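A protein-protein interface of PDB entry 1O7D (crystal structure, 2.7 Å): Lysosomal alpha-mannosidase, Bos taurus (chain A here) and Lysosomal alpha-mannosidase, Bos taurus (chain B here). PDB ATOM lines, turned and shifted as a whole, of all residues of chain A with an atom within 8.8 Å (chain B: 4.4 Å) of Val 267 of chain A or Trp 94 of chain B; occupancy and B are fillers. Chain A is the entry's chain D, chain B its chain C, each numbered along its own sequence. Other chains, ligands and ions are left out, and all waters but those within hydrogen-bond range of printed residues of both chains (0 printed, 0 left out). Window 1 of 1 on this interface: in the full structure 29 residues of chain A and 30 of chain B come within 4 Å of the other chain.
Arg 104 of chain A touches Ser 133 of chain B (NH2 to OG, 3.8 Å).
CG1 of Val 84 of chain B touches CB of Pro 265 of chain A (3.97 Å).
Pro 265 of chain A touches Trp 94 of chain B (CG to CD2, 3.1 Å).
Gln 266 of chain A touches Ile 83 of chain B.
O of Gln 266 of chain A touches CA of Val 84 of chain B (3.4 Å).
Val 267 of chain A touches Ile 83 of chain B (CA to O, 3.4 Å).
Val 267 of chain A touches Val 84 of chain B (CG2 to CG2, 3.7 Å).
Val 267 of chain A touches Trp 94 of chain B (CG2 to CZ3, 3.9 Å).
Val 268 of chain A touches Val 82 of chain B.
N of Ile 83 of chain B sits at hydrogen-bond distance from O of Val 268 of chain A (2.8 Å).
The side-chain carboxylate of Asp 93 of chain B lies within salt-bridge range of the guanidinium group of Arg 104 of chain A, 2.6 Å away.
Of the 11 printed residues of chain B, 6 touch a printed residue of chain A.
Gln 105 of chain A touches none of the printed residues of chain B.
Val 267 of chain A touches just these residues of chain B: Ile 83 (3.4 Å), Val 84 (3.7 Å) and Trp 94 (3.9 Å).
Of the printed residues of chain A, Val 84 of chain B touches Pro 265, Gln 266 and Val 267.
Val 92 of chain B touches none of the printed residues of chain A.
Trp 94 of chain B touches just these residues of chain A: Pro 265 and Val 267.
Printed residues of chain A within 4 Å of Ser 133 of chain B: Arg 104 (3.8 Å).
No residue of chain A comes within 4 Å of Ala 134 of chain B.
The backbone NH (N) of Ala 134 of chain B is in hydrogen-bond range of the backbone carbonyl oxygen (O) of Trp 94 of chain B (2.9 Å).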
ATOM      1  N   TYR A 102       1.834  30.801 -16.803  1.00  0.00           N
ATOM      2  CA  TYR A 102       0.895  30.132 -15.907  1.00  0.00           C
ATOM      3  C   TYR A 102       1.047  30.654 -14.475  1.00  0.00           C
ATOM      4  O   TYR A 102       2.002  31.342 -14.146  1.00  0.00           O
ATOM      5  CB  TYR A 102       1.157  28.623 -15.873  1.00  0.00           C
ATOM      6  CG  TYR A 102       0.631  27.835 -17.041  1.00  0.00           C
ATOM      7  CD1 TYR A 102      -0.731  27.718 -17.274  1.00  0.00           C
ATOM      8  CD2 TYR A 102       1.500  27.169 -17.898  1.00  0.00           C
ATOM      9  CE1 TYR A 102      -1.211  26.954 -18.331  1.00  0.00           C
ATOM     10  CE2 TYR A 102       1.020  26.402 -18.965  1.00  0.00           C
ATOM     11  CZ  TYR A 102      -0.335  26.304 -19.167  1.00  0.00           C
ATOM     12  OH  TYR A 102      -0.802  25.553 -20.208  1.00  0.00           O
ATOM     13  N   PRO A 103       0.076  30.338 -13.611  1.00  0.00           N
ATOM     14  CA  PRO A 103       0.028  30.716 -12.200  1.00  0.00           C
ATOM     15  C   PRO A 103       1.257  30.350 -11.365  1.00  0.00           C
ATOM     16  O   PRO A 103       1.581  29.173 -11.149  1.00  0.00           O
ATOM     17  CB  PRO A 103      -1.236  30.012 -11.725  1.00  0.00           C
ATOM     18  CG  PRO A 103      -2.151  30.317 -12.841  1.00  0.00           C
ATOM     19  CD  PRO A 103      -1.286  30.011 -14.076  1.00  0.00           C
ATOM     20  N   ARG A 104       1.939  31.392 -10.916  1.00  0.00           N
ATOM     21  CA  ARG A 104       3.095  31.239 -10.073  1.00  0.00           C
ATOM     22  C   ARG A 104       4.253  30.498 -10.710  1.00  0.00           C
ATOM     23  O   ARG A 104       5.039  29.877  -9.998  1.00  0.00           O
ATOM     24  CB  ARG A 104       2.687  30.519  -8.785  1.00  0.00           C
ATOM     25  CG  ARG A 104       1.708  31.274  -7.924  1.00  0.00           C
ATOM     26  CD  ARG A 104       1.396  30.455  -6.655  1.00  0.00           C
ATOM     27  NE  ARG A 104       0.832  29.125  -6.970  1.00  0.00           N
ATOM     28  CZ  ARG A 104      -0.317  28.906  -7.633  1.00  0.00           C
ATOM     29  NH1 ARG A 104      -1.057  29.920  -8.064  1.00  0.00           N
ATOM     30  NH2 ARG A 104      -0.732  27.664  -7.892  1.00  0.00           N
ATOM     31  N   GLN A 105       4.385  30.515 -12.027  1.00  0.00           N
ATOM     32  CA  GLN A 105       5.544  29.816 -12.563  1.00  0.00           C
ATOM     33  C   GLN A 105       6.622  30.842 -12.923  1.00  0.00           C
ATOM     34  O   GLN A 105       6.342  31.862 -13.564  1.00  0.00           O
ATOM     35  CB  GLN A 105       5.179  28.908 -13.752  1.00  0.00           C
ATOM     36  CG  GLN A 105       4.503  29.585 -14.897  1.00  0.00           C
ATOM     37  CD  GLN A 105       4.284  28.646 -16.094  1.00  0.00           C
ATOM     38  OE1 GLN A 105       4.231  27.415 -15.947  1.00  0.00           O
ATOM     39  NE2 GLN A 105       4.131  29.235 -17.284  1.00  0.00           N
ATOM     40  N   HIS A 107       9.015  30.800 -15.032  1.00  0.00           N
ATOM     41  CA  HIS A 107       9.439  30.915 -16.424  1.00  0.00           C
ATOM     42  C   HIS A 107       8.328  31.249 -17.420  1.00  0.00           C
ATOM     43  O   HIS A 107       7.144  31.171 -17.110  1.00  0.00           O
ATOM     44  CB  HIS A 107      10.074  29.621 -16.871  1.00  0.00           C
ATOM     45  CG  HIS A 107       9.143  28.457 -16.786  1.00  0.00           C
ATOM     46  ND1 HIS A 107       9.075  27.647 -15.672  1.00  0.00           N
ATOM     47  CD2 HIS A 107       8.198  28.006 -17.641  1.00  0.00           C
ATOM     48  CE1 HIS A 107       8.126  26.745 -15.849  1.00  0.00           C
ATOM     49  NE2 HIS A 107       7.575  26.938 -17.036  1.00  0.00           N
ATOM     50  N   GLU A 109       6.716  30.207 -20.963  1.00  0.00           N
ATOM     51  CA  GLU A 109       6.646  29.035 -21.828  1.00  0.00           C
ATOM     52  C   GLU A 109       6.505  29.364 -23.311  1.00  0.00           C
ATOM     53  O   GLU A 109       5.604  30.093 -23.701  1.00  0.00           O
ATOM     54  CB  GLU A 109       5.486  28.140 -21.393  1.00  0.00           C
ATOM     55  CG  GLU A 109       5.278  26.937 -22.283  1.00  0.00           C
ATOM     56  CD  GLU A 109       4.148  26.058 -21.799  1.00  0.00           C
ATOM     57  OE1 GLU A 109       4.289  25.456 -20.704  1.00  0.00           O
ATOM     58  OE2 GLU A 109       3.117  25.977 -22.511  1.00  0.00           O
ATOM     59  N   ARG A 239       8.397  22.602 -26.467  1.00  0.00           N
ATOM     60  CA  ARG A 239       8.418  23.766 -25.573  1.00  0.00           C
ATOM     61  C   ARG A 239       9.839  24.228 -25.239  1.00  0.00           C
ATOM     62  O   ARG A 239      10.793  23.455 -25.317  1.00  0.00           O
ATOM     63  CB  ARG A 239       7.674  23.466 -24.263  1.00  0.00           C
ATOM     64  CG  ARG A 239       6.349  22.730 -24.442  1.00  0.00           C
ATOM     65  CD  ARG A 239       5.479  22.784 -23.195  1.00  0.00           C
ATOM     66  NE  ARG A 239       6.217  22.507 -21.966  1.00  0.00           N
ATOM     67  CZ  ARG A 239       6.891  21.383 -21.704  1.00  0.00           C
ATOM     68  NH1 ARG A 239       6.946  20.382 -22.581  1.00  0.00           N
ATOM     69  NH2 ARG A 239       7.522  21.263 -20.546  1.00  0.00           N
ATOM     70  N   GLN A 257      14.109  23.750 -11.909  1.00  0.00           N
ATOM     71  CA  GLN A 257      13.035  23.657 -12.885  1.00  0.00           C
ATOM     72  C   GLN A 257      13.395  22.626 -13.941  1.00  0.00           C
ATOM     73  O   GLN A 257      12.518  21.952 -14.496  1.00  0.00           O
ATOM     74  CB  GLN A 257      12.792  24.998 -13.566  1.00  0.00           C
ATOM     75  CG  GLN A 257      11.661  24.915 -14.574  1.00  0.00           C
ATOM     76  CD  GLN A 257      10.304  25.000 -13.914  1.00  0.00           C
ATOM     77  OE1 GLN A 257       9.933  26.058 -13.381  1.00  0.00           O
ATOM     78  NE2 GLN A 257       9.553  23.893 -13.930  1.00  0.00           N
ATOM     79  N   MET A 260      12.277  19.522 -12.750  1.00  0.00           N
ATOM     80  CA  MET A 260      10.825  19.389 -12.777  1.00  0.00           C
ATOM     81  C   MET A 260      10.377  19.120 -14.202  1.00  0.00           C
ATOM     82  O   MET A 260       9.269  18.651 -14.444  1.00  0.00           O
ATOM     83  CB  MET A 260      10.151  20.656 -12.266  1.00  0.00           C
ATOM     84  CG  MET A 260      10.335  20.898 -10.789  1.00  0.00           C
ATOM     85  SD  MET A 260       9.319  22.293 -10.210  1.00  0.00           S
ATOM     86  CE  MET A 260      10.495  23.671 -10.239  1.00  0.00           C
ATOM     87  N   GLU A 261      11.275  19.404 -15.135  1.00  0.00           N
ATOM     88  CA  GLU A 261      11.048  19.242 -16.565  1.00  0.00           C
ATOM     89  C   GLU A 261      11.212  17.806 -17.074  1.00  0.00           C
ATOM     90  O   GLU A 261      10.420  17.332 -17.886  1.00  0.00           O
ATOM     91  CB  GLU A 261      12.009  20.177 -17.306  1.00  0.00           C
ATOM     92  CG  GLU A 261      11.781  20.313 -18.792  1.00  0.00           C
ATOM     93  CD  GLU A 261      10.339  20.572 -19.124  1.00  0.00           C
ATOM     94  OE1 GLU A 261       9.717  21.431 -18.452  1.00  0.00           O
ATOM     95  OE2 GLU A 261       9.835  19.910 -20.058  1.00  0.00           O
ATOM     96  N   LEU A 263      11.625  14.990 -14.859  1.00  0.00           N
ATOM     97  CA  LEU A 263      10.864  14.136 -13.951  1.00  0.00           C
ATOM     98  C   LEU A 263       9.549  14.835 -13.680  1.00  0.00           C
ATOM     99  O   LEU A 263       9.246  15.197 -12.545  1.00  0.00           O
ATOM    100  CB  LEU A 263      11.629  13.939 -12.653  1.00  0.00           C
ATOM    101  CG  LEU A 263      12.820  13.010 -12.823  1.00  0.00           C
ATOM    102  CD1 LEU A 263      13.523  12.820 -11.489  1.00  0.00           C
ATOM    103  CD2 LEU A 263      12.313  11.679 -13.378  1.00  0.00           C
ATOM    104  N   ALA A 264       8.776  15.033 -14.741  1.00  0.00           N
ATOM    105  CA  ALA A 264       7.503  15.723 -14.652  1.00  0.00           C
ATOM    106  C   ALA A 264       6.393  14.838 -14.099  1.00  0.00           C
ATOM    107  O   ALA A 264       6.574  13.637 -13.924  1.00  0.00           O
ATOM    108  CB  ALA A 264       7.132  16.251 -16.013  1.00  0.00           C
ATOM    109  N   PRO A 265       5.224  15.428 -13.810  1.00  0.00           N
ATOM    110  CA  PRO A 265       4.136  14.614 -13.274  1.00  0.00           C
ATOM    111  C   PRO A 265       3.416  13.782 -14.336  1.00  0.00           C
ATOM    112  O   PRO A 265       3.353  14.176 -15.497  1.00  0.00           O
ATOM    113  CB  PRO A 265       3.253  15.649 -12.585  1.00  0.00           C
ATOM    114  CG  PRO A 265       3.450  16.848 -13.401  1.00  0.00           C
ATOM    115  CD  PRO A 265       4.909  16.863 -13.711  1.00  0.00           C
ATOM    116  N   GLN A 266       2.910  12.615 -13.932  1.00  0.00           N
ATOM    117  CA  GLN A 266       2.190  11.713 -14.820  1.00  0.00           C
ATOM    118  C   GLN A 266       0.694  11.751 -14.475  1.00  0.00           C
ATOM    119  O   GLN A 266       0.306  11.775 -13.305  1.00  0.00           O
ATOM    120  CB  GLN A 266       2.737  10.291 -14.672  1.00  0.00           C
ATOM    121  CG  GLN A 266       2.006   9.221 -15.472  1.00  0.00           C
ATOM    122  CD  GLN A 266       2.077   9.462 -16.966  1.00  0.00           C
ATOM    123  OE1 GLN A 266       3.133   9.820 -17.493  1.00  0.00           O
ATOM    124  NE2 GLN A 266       0.950   9.254 -17.665  1.00  0.00           N
ATOM    125  N   VAL A 267      -0.146  11.776 -15.500  1.00  0.00           N
ATOM    126  CA  VAL A 267      -1.571  11.820 -15.284  1.00  0.00           C
ATOM    127  C   VAL A 267      -2.231  10.577 -15.810  1.00  0.00           C
ATOM    128  O   VAL A 267      -1.935  10.136 -16.921  1.00  0.00           O
ATOM    129  CB  VAL A 267      -2.183  13.009 -15.977  1.00  0.00           C
ATOM    130  CG1 VAL A 267      -3.660  12.792 -16.166  1.00  0.00           C
ATOM    131  CG2 VAL A 267      -1.931  14.236 -15.167  1.00  0.00           C
ATOM    132  N   VAL A 268      -3.113  10.011 -14.987  1.00  0.00           N
ATOM    133  CA  VAL A 268      -3.873   8.817 -15.334  1.00  0.00           C
ATOM    134  C   VAL A 268      -5.330   9.110 -14.975  1.00  0.00           C
ATOM    135  O   VAL A 268      -5.625   9.693 -13.926  1.00  0.00           O
ATOM    136  CB  VAL A 268      -3.379   7.555 -14.575  1.00  0.00           C
ATOM    137  CG1 VAL A 268      -3.612   7.718 -13.101  1.00  0.00           C
ATOM    138  CG2 VAL A 268      -4.100   6.316 -15.088  1.00  0.00           C
ATOM    139  N   LEU A 269      -6.236   8.703 -15.854  1.00  0.00           N
ATOM    140  CA  LEU A 269      -7.638   8.967 -15.645  1.00  0.00           C
ATOM    141  C   LEU A 269      -8.433   7.735 -15.326  1.00  0.00           C
ATOM    142  O   LEU A 269      -8.052   6.619 -15.675  1.00  0.00           O
ATOM    143  CB  LEU A 269      -8.218   9.635 -16.882  1.00  0.00           C
ATOM    144  CG  LEU A 269      -7.317  10.730 -17.445  1.00  0.00           C
ATOM    145  CD1 LEU A 269      -7.914  11.245 -18.747  1.00  0.00           C
ATOM    146  CD2 LEU A 269      -7.148  11.845 -16.422  1.00  0.00           C
ATOM    147  N   ALA A 270      -9.555   7.969 -14.658  1.00  0.00           N
ATOM    148  CA  ALA A 270     -10.479   6.922 -14.259  1.00  0.00           C
ATOM    149  C   ALA A 270     -11.888   7.511 -14.287  1.00  0.00           C
ATOM    150  O   ALA A 270     -12.133   8.618 -13.791  1.00  0.00           O
ATOM    151  CB  ALA A 270     -10.140   6.431 -12.861  1.00  0.00           C
ATOM    152  N   VAL B  82      -9.086  12.559 -12.128  1.00  0.00           N
ATOM    153  CA  VAL B  82      -7.735  12.836 -12.588  1.00  0.00           C
ATOM    154  C   VAL B  82      -6.705  12.436 -11.520  1.00  0.00           C
ATOM    155  O   VAL B  82      -6.599  13.083 -10.475  1.00  0.00           O
ATOM    156  CB  VAL B  82      -7.558  14.333 -12.852  1.00  0.00           C
ATOM    157  CG1 VAL B  82      -6.193  14.605 -13.433  1.00  0.00           C
ATOM    158  CG2 VAL B  82      -8.664  14.829 -13.751  1.00  0.00           C
ATOM    159  N   ILE B  83      -5.954  11.370 -11.757  1.00  0.00           N
ATOM    160  CA  ILE B  83      -4.931  10.993 -10.785  1.00  0.00           C
ATOM    161  C   ILE B  83      -3.625  11.568 -11.296  1.00  0.00           C
ATOM    162  O   ILE B  83      -3.176  11.187 -12.369  1.00  0.00           O
ATOM    163  CB  ILE B  83      -4.731   9.457 -10.669  1.00  0.00           C
ATOM    164  CG1 ILE B  83      -6.024   8.771 -10.255  1.00  0.00           C
ATOM    165  CG2 ILE B  83      -3.663   9.156  -9.644  1.00  0.00           C
ATOM    166  CD1 ILE B  83      -7.017   8.697 -11.360  1.00  0.00           C
ATOM    167  N   VAL B  84      -3.021  12.482 -10.547  1.00  0.00           N
ATOM    168  CA  VAL B  84      -1.752  13.066 -10.972  1.00  0.00           C
ATOM    169  C   VAL B  84      -0.609  12.583 -10.078  1.00  0.00           C
ATOM    170  O   VAL B  84      -0.582  12.895  -8.894  1.00  0.00           O
ATOM    171  CB  VAL B  84      -1.802  14.603 -10.932  1.00  0.00           C
ATOM    172  CG1 VAL B  84      -0.538  15.176 -11.490  1.00  0.00           C
ATOM    173  CG2 VAL B  84      -2.963  15.096 -11.742  1.00  0.00           C
ATOM    174  N   VAL B  92       4.570  19.207  -5.748  1.00  0.00           N
ATOM    175  CA  VAL B  92       4.370  19.933  -7.000  1.00  0.00           C
ATOM    176  C   VAL B  92       3.009  20.617  -6.972  1.00  0.00           C
ATOM    177  O   VAL B  92       2.056  20.111  -6.373  1.00  0.00           O
ATOM    178  CB  VAL B  92       4.438  18.999  -8.248  1.00  0.00           C
ATOM    179  CG1 VAL B  92       3.906  19.723  -9.470  1.00  0.00           C
ATOM    180  CG2 VAL B  92       5.882  18.584  -8.508  1.00  0.00           C
ATOM    181  N   ASP B  93       2.956  21.792  -7.593  1.00  0.00           N
ATOM    182  CA  ASP B  93       1.738  22.582  -7.730  1.00  0.00           C
ATOM    183  C   ASP B  93       1.764  22.738  -9.229  1.00  0.00           C
ATOM    184  O   ASP B  93       2.218  23.749  -9.743  1.00  0.00           O
ATOM    185  CB  ASP B  93       1.879  23.951  -7.052  1.00  0.00           C
ATOM    186  CG  ASP B  93       0.639  24.835  -7.238  1.00  0.00           C
ATOM    187  OD1 ASP B  93      -0.175  24.546  -8.158  1.00  0.00           O
ATOM    188  OD2 ASP B  93       0.485  25.828  -6.474  1.00  0.00           O
ATOM    189  N   TRP B  94       1.296  21.702  -9.913  1.00  0.00           N
ATOM    190  CA  TRP B  94       1.285  21.618 -11.375  1.00  0.00           C
ATOM    191  C   TRP B  94      -0.068  21.843 -12.065  1.00  0.00           C
ATOM    192  O   TRP B  94      -1.105  21.410 -11.581  1.00  0.00           O
ATOM    193  CB  TRP B  94       1.810  20.241 -11.736  1.00  0.00           C
ATOM    194  CG  TRP B  94       2.164  20.043 -13.147  1.00  0.00           C
ATOM    195  CD1 TRP B  94       3.250  20.555 -13.814  1.00  0.00           C
ATOM    196  CD2 TRP B  94       1.495  19.187 -14.062  1.00  0.00           C
ATOM    197  NE1 TRP B  94       3.298  20.051 -15.093  1.00  0.00           N
ATOM    198  CE2 TRP B  94       2.228  19.208 -15.270  1.00  0.00           C
ATOM    199  CE3 TRP B  94       0.344  18.396 -13.980  1.00  0.00           C
ATOM    200  CZ2 TRP B  94       1.845  18.463 -16.387  1.00  0.00           C
ATOM    201  CZ3 TRP B  94      -0.038  17.655 -15.092  1.00  0.00           C
ATOM    202  CH2 TRP B  94       0.713  17.694 -16.281  1.00  0.00           C
ATOM    203  N   MET B  95      -0.054  22.495 -13.220  1.00  0.00           N
ATOM    204  CA  MET B  95      -1.308  22.759 -13.945  1.00  0.00           C
ATOM    205  C   MET B  95      -1.760  21.601 -14.822  1.00  0.00           C
ATOM    206  O   MET B  95      -0.979  21.085 -15.627  1.00  0.00           O
ATOM    207  CB  MET B  95      -1.180  24.003 -14.832  1.00  0.00           C
ATOM    208  CG  MET B  95      -1.662  25.306 -14.215  1.00  0.00           C
ATOM    209  SD  MET B  95      -3.431  25.352 -13.868  1.00  0.00           S
ATOM    210  CE  MET B  95      -4.124  25.006 -15.466  1.00  0.00           C
ATOM    211  N   VAL B  96      -3.015  21.190 -14.664  1.00  0.00           N
ATOM    212  CA  VAL B  96      -3.564  20.115 -15.488  1.00  0.00           C
ATOM    213  C   VAL B  96      -4.253  20.757 -16.697  1.00  0.00           C
ATOM    214  O   VAL B  96      -4.849  21.824 -16.578  1.00  0.00           O
ATOM    215  CB  VAL B  96      -4.610  19.256 -14.722  1.00  0.00           C
ATOM    216  CG1 VAL B  96      -5.080  18.112 -15.606  1.00  0.00           C
ATOM    217  CG2 VAL B  96      -4.013  18.691 -13.453  1.00  0.00           C
ATOM    218  N   PHE B 132      -6.834  23.465 -14.150  1.00  0.00           N
ATOM    219  CA  PHE B 132      -6.869  23.609 -12.691  1.00  0.00           C
ATOM    220  C   PHE B 132      -5.529  23.228 -12.053  1.00  0.00           C
ATOM    221  O   PHE B 132      -4.718  22.529 -12.669  1.00  0.00           O
ATOM    222  CB  PHE B 132      -8.011  22.785 -12.076  1.00  0.00           C
ATOM    223  CG  PHE B 132      -7.846  21.299 -12.207  1.00  0.00           C
ATOM    224  CD1 PHE B 132      -7.040  20.589 -11.321  1.00  0.00           C
ATOM    225  CD2 PHE B 132      -8.508  20.603 -13.214  1.00  0.00           C
ATOM    226  CE1 PHE B 132      -6.893  19.199 -11.431  1.00  0.00           C
ATOM    227  CE2 PHE B 132      -8.368  19.214 -13.335  1.00  0.00           C
ATOM    228  CZ  PHE B 132      -7.552  18.510 -12.436  1.00  0.00           C
ATOM    229  N   SER B 133      -5.293  23.708 -10.831  1.00  0.00           N
ATOM    230  CA  SER B 133      -4.047  23.413 -10.129  1.00  0.00           C
ATOM    231  C   SER B 133      -4.152  22.087  -9.418  1.00  0.00           C
ATOM    232  O   SER B 133      -5.167  21.768  -8.807  1.00  0.00           O
ATOM    233  CB  SER B 133      -3.704  24.485  -9.093  1.00  0.00           C
ATOM    234  OG  SER B 133      -3.394  25.724  -9.703  1.00  0.00           O
ATOM    235  N   ALA B 134      -3.096  21.301  -9.519  1.00  0.00           N
ATOM    236  CA  ALA B 134      -3.063  20.014  -8.858  1.00  0.00           C
ATOM    237  C   ALA B 134      -1.868  19.981  -7.902  1.00  0.00           C
ATOM    238  O   ALA B 134      -0.714  19.934  -8.341  1.00  0.00           O
ATOM    239  CB  ALA B 134      -2.947  18.894  -9.886  1.00  0.00           C
